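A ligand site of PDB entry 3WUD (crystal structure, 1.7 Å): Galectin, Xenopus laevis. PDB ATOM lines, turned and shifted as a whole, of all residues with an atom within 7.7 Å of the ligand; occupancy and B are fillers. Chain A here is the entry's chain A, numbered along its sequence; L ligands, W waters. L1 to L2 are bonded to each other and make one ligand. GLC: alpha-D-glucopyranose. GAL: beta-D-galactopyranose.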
ATOM      1  N   SER A  32     -13.545  27.809   7.231  1.00  0.00           N
ATOM      2  CA  SER A  32     -13.155  26.404   7.433  1.00  0.00           C
ATOM      3  C   SER A  32     -11.992  26.070   6.447  1.00  0.00           C
ATOM      4  O   SER A  32     -11.695  26.864   5.531  1.00  0.00           O
ATOM      5  CB  SER A  32     -14.343  25.448   7.140  1.00  0.00           C
ATOM      6  OG  SER A  32     -14.722  25.566   5.816  1.00  0.00           O
ATOM      7  N   PHE A  33     -11.347  24.976   6.628  1.00  0.00           N
ATOM      8  CA  PHE A  33     -10.434  24.448   5.601  1.00  0.00           C
ATOM      9  C   PHE A  33     -10.532  22.889   5.633  1.00  0.00           C
ATOM     10  O   PHE A  33     -11.070  22.322   6.602  1.00  0.00           O
ATOM     11  CB  PHE A  33      -8.988  24.942   5.821  1.00  0.00           C
ATOM     12  CG  PHE A  33      -8.317  24.425   7.080  1.00  0.00           C
ATOM     13  CD1 PHE A  33      -7.474  23.317   7.040  1.00  0.00           C
ATOM     14  CD2 PHE A  33      -8.446  25.090   8.310  1.00  0.00           C
ATOM     15  CE1 PHE A  33      -6.848  22.836   8.166  1.00  0.00           C
ATOM     16  CE2 PHE A  33      -7.793  24.642   9.444  1.00  0.00           C
ATOM     17  CZ  PHE A  33      -7.004  23.516   9.374  1.00  0.00           C
ATOM     18  N   ALA A  34     -10.097  22.211   4.560  1.00  0.00           N
ATOM     19  CA  ALA A  34     -10.262  20.753   4.542  1.00  0.00           C
ATOM     20  C   ALA A  34      -8.998  20.186   3.949  1.00  0.00           C
ATOM     21  O   ALA A  34      -8.434  20.790   3.001  1.00  0.00           O
ATOM     22  CB  ALA A  34     -11.500  20.326   3.730  1.00  0.00           C
ATOM     23  N   ASN A  36      -8.057  16.372   2.485  1.00  0.00           N
ATOM     24  CA  ASN A  36      -8.524  15.073   2.091  1.00  0.00           C
ATOM     25  C   ASN A  36      -7.399  14.100   1.743  1.00  0.00           C
ATOM     26  O   ASN A  36      -6.520  14.479   1.014  1.00  0.00           O
ATOM     27  CB  ASN A  36      -9.353  15.302   0.871  1.00  0.00           C
ATOM     28  CG  ASN A  36     -10.532  16.206   1.123  1.00  0.00           C
ATOM     29  OD1 ASN A  36     -11.291  16.004   2.079  1.00  0.00           O
ATOM     30  ND2 ASN A  36     -10.691  17.186   0.282  1.00  0.00           N
ATOM     31  N   HIS A  47     -11.691  13.018   5.187  1.00  0.00           N
ATOM     32  CA  HIS A  47     -11.977  14.385   4.931  1.00  0.00           C
ATOM     33  C   HIS A  47     -11.885  14.995   6.309  1.00  0.00           C
ATOM     34  O   HIS A  47     -12.708  14.659   7.193  1.00  0.00           O
ATOM     35  CB  HIS A  47     -13.372  14.551   4.327  1.00  0.00           C
ATOM     36  CG  HIS A  47     -13.889  15.973   4.285  1.00  0.00           C
ATOM     37  ND1 HIS A  47     -13.459  16.913   3.376  1.00  0.00           N
ATOM     38  CD2 HIS A  47     -14.861  16.552   5.012  1.00  0.00           C
ATOM     39  CE1 HIS A  47     -14.171  18.024   3.546  1.00  0.00           C
ATOM     40  NE2 HIS A  47     -15.064  17.800   4.488  1.00  0.00           N
ATOM     41  N   PHE A  48     -10.872  15.822   6.504  1.00  0.00           N
ATOM     42  CA  PHE A  48     -10.499  16.442   7.757  1.00  0.00           C
ATOM     43  C   PHE A  48     -10.828  17.927   7.655  1.00  0.00           C
ATOM     44  O   PHE A  48     -10.228  18.643   6.848  1.00  0.00           O
ATOM     45  CB  PHE A  48      -8.997  16.265   7.961  1.00  0.00           C
ATOM     46  CG  PHE A  48      -8.458  16.944   9.174  1.00  0.00           C
ATOM     47  CD1 PHE A  48      -8.559  16.335  10.425  1.00  0.00           C
ATOM     48  CD2 PHE A  48      -7.840  18.184   9.075  1.00  0.00           C
ATOM     49  CE1 PHE A  48      -8.047  16.946  11.545  1.00  0.00           C
ATOM     50  CE2 PHE A  48      -7.330  18.841  10.212  1.00  0.00           C
ATOM     51  CZ  PHE A  48      -7.472  18.209  11.450  1.00  0.00           C
ATOM     52  N   ASN A  49     -11.899  18.365   8.317  1.00  0.00           N
ATOM     53  CA  ASN A  49     -12.484  19.674   8.095  1.00  0.00           C
ATOM     54  C   ASN A  49     -12.714  20.568   9.390  1.00  0.00           C
ATOM     55  O   ASN A  49     -13.807  20.566   9.933  1.00  0.00           O
ATOM     56  CB  ASN A  49     -13.825  19.436   7.390  1.00  0.00           C
ATOM     57  CG  ASN A  49     -14.530  20.717   6.913  1.00  0.00           C
ATOM     58  OD1 ASN A  49     -15.743  20.716   6.831  1.00  0.00           O
ATOM     59  ND2 ASN A  49     -13.797  21.762   6.578  1.00  0.00           N
ATOM     60  N   ARG A  51     -13.628  23.664  11.254  1.00  0.00           N
ATOM     61  CA  ARG A  51     -14.611  24.611  10.974  1.00  0.00           C
ATOM     62  C   ARG A  51     -14.583  25.694  12.076  1.00  0.00           C
ATOM     63  O   ARG A  51     -14.894  25.393  13.264  1.00  0.00           O
ATOM     64  CB  ARG A  51     -16.000  23.977  10.998  1.00  0.00           C
ATOM     65  CG  ARG A  51     -16.171  22.939   9.899  1.00  0.00           C
ATOM     66  CD  ARG A  51     -17.586  22.390   9.815  1.00  0.00           C
ATOM     67  NE  ARG A  51     -17.705  21.428   8.691  1.00  0.00           N
ATOM     68  CZ  ARG A  51     -18.783  20.654   8.497  1.00  0.00           C
ATOM     69  NH1 ARG A  51     -19.834  20.772   9.281  1.00  0.00           N
ATOM     70  NH2 ARG A  51     -18.847  19.821   7.467  1.00  0.00           N
ATOM     71  N   HIS A  54     -18.875  27.196  10.098  1.00  0.00           N
ATOM     72  CA  HIS A  54     -19.290  26.608   8.848  1.00  0.00           C
ATOM     73  C   HIS A  54     -20.286  25.535   9.108  1.00  0.00           C
ATOM     74  O   HIS A  54     -20.165  24.777  10.030  1.00  0.00           O
ATOM     75  CB  HIS A  54     -18.032  26.106   8.081  1.00  0.00           C
ATOM     76  CG  HIS A  54     -18.358  25.461   6.781  1.00  0.00           C
ATOM     77  ND1 HIS A  54     -18.994  26.115   5.752  1.00  0.00           N
ATOM     78  CD2 HIS A  54     -18.096  24.207   6.338  1.00  0.00           C
ATOM     79  CE1 HIS A  54     -19.174  25.270   4.745  1.00  0.00           C
ATOM     80  NE2 HIS A  54     -18.605  24.122   5.060  1.00  0.00           N
ATOM     81  N   GLU A  55     -21.337  25.518   8.322  1.00  0.00           N
ATOM     82  CA  GLU A  55     -22.432  24.537   8.495  1.00  0.00           C
ATOM     83  C   GLU A  55     -22.971  24.505   9.916  1.00  0.00           C
ATOM     84  O   GLU A  55     -23.330  23.453  10.362  1.00  0.00           O
ATOM     85  CB  GLU A  55     -21.998  23.114   8.056  1.00  0.00           C
ATOM     86  CG  GLU A  55     -21.479  23.021   6.632  1.00  0.00           C
ATOM     87  CD  GLU A  55     -22.576  22.968   5.571  1.00  0.00           C
ATOM     88  OE1 GLU A  55     -22.239  22.776   4.372  1.00  0.00           O
ATOM     89  OE2 GLU A  55     -23.758  23.059   5.923  1.00  0.00           O
ATOM     90  N   GLY A  56     -23.035  25.650  10.609  1.00  0.00           N
ATOM     91  CA  GLY A  56     -23.468  25.739  12.027  1.00  0.00           C
ATOM     92  C   GLY A  56     -22.505  25.263  13.117  1.00  0.00           C
ATOM     93  O   GLY A  56     -22.844  25.268  14.354  1.00  0.00           O
ATOM     94  N   ASP A  57     -21.280  24.895  12.707  1.00  0.00           N
ATOM     95  CA  ASP A  57     -20.264  24.375  13.614  1.00  0.00           C
ATOM     96  C   ASP A  57     -19.245  25.511  13.870  1.00  0.00           C
ATOM     97  O   ASP A  57     -18.878  26.203  12.893  1.00  0.00           O
ATOM     98  CB  ASP A  57     -19.542  23.162  13.017  1.00  0.00           C
ATOM     99  CG  ASP A  57     -20.456  21.999  12.853  1.00  0.00           C
ATOM    100  OD1 ASP A  57     -21.239  21.713  13.771  1.00  0.00           O
ATOM    101  OD2 ASP A  57     -20.417  21.426  11.758  1.00  0.00           O
ATOM    102  N   ILE A  62     -14.778  18.511  11.894  1.00  0.00           N
ATOM    103  CA  ILE A  62     -15.705  17.472  11.398  1.00  0.00           C
ATOM    104  C   ILE A  62     -14.833  16.575  10.532  1.00  0.00           C
ATOM    105  O   ILE A  62     -14.061  17.089   9.724  1.00  0.00           O
ATOM    106  CB  ILE A  62     -16.761  18.118  10.532  1.00  0.00           C
ATOM    107  CG1 ILE A  62     -17.838  18.760  11.401  1.00  0.00           C
ATOM    108  CG2 ILE A  62     -17.445  17.071   9.624  1.00  0.00           C
ATOM    109  CD1 ILE A  62     -17.392  19.544  12.613  1.00  0.00           C
ATOM    110  N   CYS A  63     -14.837  15.259  10.768  1.00  0.00           N
ATOM    111  CA  CYS A  63     -14.185  14.325   9.833  1.00  0.00           C
ATOM    112  C   CYS A  63     -15.251  13.427   9.202  1.00  0.00           C
ATOM    113  O   CYS A  63     -16.297  13.098   9.806  1.00  0.00           O
ATOM    114  CB  CYS A  63     -13.209  13.447  10.574  1.00  0.00           C
ATOM    115  SG  CYS A  63     -11.773  14.427  11.186  1.00  0.00           S
ATOM    116  N   ASN A  64     -14.989  13.001   7.982  1.00  0.00           N
ATOM    117  CA  ASN A  64     -15.833  12.033   7.340  1.00  0.00           C
ATOM    118  C   ASN A  64     -15.051  11.281   6.284  1.00  0.00           C
ATOM    119  O   ASN A  64     -13.933  11.611   5.982  1.00  0.00           O
ATOM    120  CB  ASN A  64     -17.005  12.766   6.660  1.00  0.00           C
ATOM    121  CG  ASN A  64     -18.259  11.872   6.543  1.00  0.00           C
ATOM    122  OD1 ASN A  64     -18.199  10.692   6.606  1.00  0.00           O
ATOM    123  ND2 ASN A  64     -19.374  12.456   6.258  1.00  0.00           N
ATOM    124  N   SER A  65     -15.622  10.232   5.779  1.00  0.00           N
ATOM    125  CA  SER A  65     -15.110   9.503   4.639  1.00  0.00           C
ATOM    126  C   SER A  65     -15.926   9.817   3.425  1.00  0.00           C
ATOM    127  O   SER A  65     -17.103  10.225   3.540  1.00  0.00           O
ATOM    128  CB  SER A  65     -15.187   7.981   4.913  1.00  0.00           C
ATOM    129  OG  SER A  65     -16.501   7.503   5.195  1.00  0.00           O
ATOM    130  N   TRP A  71     -20.661  10.746   0.906  1.00  0.00           N
ATOM    131  CA  TRP A  71     -20.248  10.936   2.293  1.00  0.00           C
ATOM    132  C   TRP A  71     -20.657   9.753   3.222  1.00  0.00           C
ATOM    133  O   TRP A  71     -21.791   9.238   3.169  1.00  0.00           O
ATOM    134  CB  TRP A  71     -20.759  12.261   2.893  1.00  0.00           C
ATOM    135  CG  TRP A  71     -20.226  13.479   2.238  1.00  0.00           C
ATOM    136  CD1 TRP A  71     -20.947  14.436   1.498  1.00  0.00           C
ATOM    137  CD2 TRP A  71     -18.866  13.881   2.167  1.00  0.00           C
ATOM    138  NE1 TRP A  71     -20.082  15.370   1.037  1.00  0.00           N
ATOM    139  CE2 TRP A  71     -18.821  15.101   1.489  1.00  0.00           C
ATOM    140  CE3 TRP A  71     -17.711  13.419   2.775  1.00  0.00           C
ATOM    141  CZ2 TRP A  71     -17.613  15.782   1.257  1.00  0.00           C
ATOM    142  CZ3 TRP A  71     -16.533  14.108   2.568  1.00  0.00           C
ATOM    143  CH2 TRP A  71     -16.469  15.242   1.843  1.00  0.00           C
ATOM    144  N   GLY A  72     -19.763   9.361   4.133  1.00  0.00           N
ATOM    145  CA  GLY A  72     -20.103   8.471   5.221  1.00  0.00           C
ATOM    146  C   GLY A  72     -20.700   9.141   6.436  1.00  0.00           C
ATOM    147  O   GLY A  72     -21.324  10.196   6.342  1.00  0.00           O
ATOM    148  N   THR A  73     -20.535   8.514   7.569  1.00  0.00           N
ATOM    149  CA  THR A  73     -20.968   9.048   8.867  1.00  0.00           C
ATOM    150  C   THR A  73     -19.956  10.067   9.444  1.00  0.00           C
ATOM    151  O   THR A  73     -18.777   9.693   9.630  1.00  0.00           O
ATOM    152  CB  THR A  73     -21.163   7.889   9.861  1.00  0.00           C
ATOM    153  OG1 THR A  73     -22.180   7.024   9.314  1.00  0.00           O
ATOM    154  CG2 THR A  73     -21.653   8.386  11.246  1.00  0.00           C
ATOM    155  N   GLU A  74     -20.399  11.314   9.777  1.00  0.00           N
ATOM    156  CA  GLU A  74     -19.454  12.263  10.323  1.00  0.00           C
ATOM    157  C   GLU A  74     -18.966  11.892  11.715  1.00  0.00           C
ATOM    158  O   GLU A  74     -19.744  11.352  12.507  1.00  0.00           O
ATOM    159  CB  GLU A  74     -20.094  13.643  10.452  1.00  0.00           C
ATOM    160  CG  GLU A  74     -20.281  14.381   9.160  1.00  0.00           C
ATOM    161  CD  GLU A  74     -20.964  15.754   9.301  1.00  0.00           C
ATOM    162  OE1 GLU A  74     -21.342  16.186  10.390  1.00  0.00           O
ATOM    163  OE2 GLU A  74     -21.049  16.428   8.303  1.00  0.00           O
ATOM    164  N   GLN A  75     -17.715  12.246  11.980  1.00  0.00           N
ATOM    165  CA  GLN A  75     -17.111  12.181  13.324  1.00  0.00           C
ATOM    166  C   GLN A  75     -16.783  13.645  13.739  1.00  0.00           C
ATOM    167  O   GLN A  75     -16.147  14.400  12.998  1.00  0.00           O
ATOM    168  CB  GLN A  75     -15.883  11.262  13.317  1.00  0.00           C
ATOM    169  CG  GLN A  75     -15.338  10.991  14.700  1.00  0.00           C
ATOM    170  CD  GLN A  75     -14.149  10.054  14.664  1.00  0.00           C
ATOM    171  OE1 GLN A  75     -14.282   8.880  14.258  1.00  0.00           O
ATOM    172  NE2 GLN A  75     -12.997  10.545  15.073  1.00  0.00           N
ATOM    173  N   ARG A  76     -17.315  14.055  14.887  1.00  0.00           N
ATOM    174  CA  ARG A  76     -17.113  15.407  15.375  1.00  0.00           C
ATOM    175  C   ARG A  76     -16.113  15.437  16.566  1.00  0.00           C
ATOM    176  O   ARG A  76     -16.270  14.708  17.573  1.00  0.00           O
ATOM    177  CB  ARG A  76     -18.442  16.092  15.721  1.00  0.00           C
ATOM    178  CG  ARG A  76     -18.947  17.113  14.710  1.00  0.00           C
ATOM    179  CD  ARG A  76     -20.336  17.726  15.019  1.00  0.00           C
ATOM    180  NE  ARG A  76     -20.867  18.473  13.848  1.00  0.00           N
ATOM    181  CZ  ARG A  76     -21.404  17.900  12.751  1.00  0.00           C
ATOM    182  NH1 ARG A  76     -21.554  16.571  12.712  1.00  0.00           N
ATOM    183  NH2 ARG A  76     -21.841  18.662  11.710  1.00  0.00           N
ATOM    184  N   ASP A 126      -8.180  22.484   0.678  1.00  0.00           N
ATOM    185  CA  ASP A 126      -8.968  23.630   0.269  1.00  0.00           C
ATOM    186  C   ASP A 126      -9.051  24.557   1.510  1.00  0.00           C
ATOM    187  O   ASP A 126      -9.176  24.096   2.620  1.00  0.00           O
ATOM    188  CB  ASP A 126     -10.366  23.165  -0.176  1.00  0.00           C
ATOM    189  CG  ASP A 126     -11.220  24.271  -0.801  1.00  0.00           C
ATOM    190  OD1 ASP A 126     -10.725  25.285  -1.408  1.00  0.00           O
ATOM    191  OD2 ASP A 126     -12.450  24.097  -0.687  1.00  0.00           O
HETATM  192  C1  GLC L   1     -25.205  18.239   7.637  1.00  0.00           C
HETATM  193  C2  GLC L   1     -23.971  18.652   8.400  1.00  0.00           C
HETATM  194  C3  GLC L   1     -22.823  19.193   7.598  1.00  0.00           C
HETATM  195  C4  GLC L   1     -22.822  18.751   6.122  1.00  0.00           C
HETATM  196  C5  GLC L   1     -24.189  18.886   5.448  1.00  0.00           C
HETATM  197  C6  GLC L   1     -24.267  18.127   4.166  1.00  0.00           C
HETATM  198  O1  GLC L   1     -26.412  18.477   8.321  1.00  0.00           O
HETATM  199  O2  GLC L   1     -24.160  19.397   9.580  1.00  0.00           O
HETATM  200  O3  GLC L   1     -21.643  18.816   8.324  1.00  0.00           O
HETATM  201  O4  GLC L   1     -21.928  19.610   5.508  1.00  0.00           O
HETATM  202  O5  GLC L   1     -25.229  18.379   6.228  1.00  0.00           O
HETATM  203  O6  GLC L   1     -25.565  18.400   3.651  1.00  0.00           O
HETATM  204  C1  GAL L   2     -20.983  18.860   4.687  1.00  0.00           C
HETATM  205  C2  GAL L   2     -20.095  19.826   3.901  1.00  0.00           C
HETATM  206  C3  GAL L   2     -19.008  19.125   3.080  1.00  0.00           C
HETATM  207  C4  GAL L   2     -18.294  18.113   3.990  1.00  0.00           C
HETATM  208  C5  GAL L   2     -19.331  17.230   4.694  1.00  0.00           C
HETATM  209  C6  GAL L   2     -18.755  16.188   5.636  1.00  0.00           C
HETATM  210  O2  GAL L   2     -20.892  20.559   2.990  1.00  0.00           O
HETATM  211  O3  GAL L   2     -18.167  20.107   2.492  1.00  0.00           O
HETATM  212  O4  GAL L   2     -17.515  18.816   4.975  1.00  0.00           O
HETATM  213  O5  GAL L   2     -20.247  17.976   5.503  1.00  0.00           O
HETATM  214  O6  GAL L   2     -19.736  15.375   6.259  1.00  0.00           O
HETATM  215  O   HOH W   1     -16.703  21.674   4.327  1.00  0.00           O
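An oxygen (O2) of GLC L1 is in hydrogen-bond range of the guanidinium group of Arg 76 (3.2 Å).
A ring nitrogen (NE2) of His 47 is in hydrogen-bond range of an oxygen (O4) of GAL L2 (2.7 Å).
OE1 of Glu 55 sits at hydrogen-bond distance from O2 of GAL L2 (2.9 Å).
The side-chain amide oxygen (OD1) of Asn 49 lies within hydrogen-bond range of an oxygen (O4) of GAL L2 (3.2 Å).
O3 of GLC L1 lies within hydrogen-bond range of OE2 of Glu 74.
The side-chain amide nitrogen (ND2) of Asn 64 lies within hydrogen-bond range of an oxygen (O6) of GAL L2 (2.9 Å).
O3 of GLC L1 lies within hydrogen-bond range of NH1 of Arg 51, at 2.8 Å.
The side-chain amide nitrogen (ND2) of Asn 49 lies within hydrogen-bond range of the backbone carbonyl oxygen (O) of Phe 33, 2.8 Å away.
The guanidinium group (NH2) of Arg 76 lies within salt-bridge range of the side-chain carboxylate (OD2) of Asp 57.
The side-chain amide nitrogen (ND2) of Asn 64 is in hydrogen-bond range of the backbone carbonyl oxygen (O) of Gly 72, 3.0 Å away.
The backbone NH (N) of His 47 is in hydrogen-bond range of the backbone carbonyl oxygen (O) of Asn 64, 2.8 Å away.
The side-chain carboxylate of Glu 74 is in salt-bridge range of the guanidinium group of Arg 76, 2.8 Å away.
The side-chain amide oxygen (OD1) of Asn 64 sits close to the backbone carbonyl oxygen (O) of Thr 73 (3.2 Å).
The guanidinium group (NH1) of Arg 51 is in salt-bridge range of the side-chain carboxylate (OD2) of Asp 57 (2.6 Å).
A ring nitrogen (ND1) of His 47 lies within hydrogen-bond range of the side-chain amide oxygen (OD1) of Asn 36, at 2.7 Å.
Residues that only touch the ligand: Trp 71 (3.7 Å).
Hydrophobic or aromatic side chains that line the ligand: His 47 and Trp 71.
Within 4 Å of the ligand: His 47, Asn 49, Arg 51, Glu 55, Asn 64, Trp 71, Glu 74 and Arg 76.
Along chain A the residues within 4 Å of the ligand span positions 47 to 76.
The nearest printed residue that does not touch the ligand is Ile 62 (4.3 Å).
Water W1 lies within hydrogen-bond range of O3 of GAL L2 (2.8 Å), OD1 of Asn 49 (2.8 Å) and NE2 of His 54 (3.2 Å).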
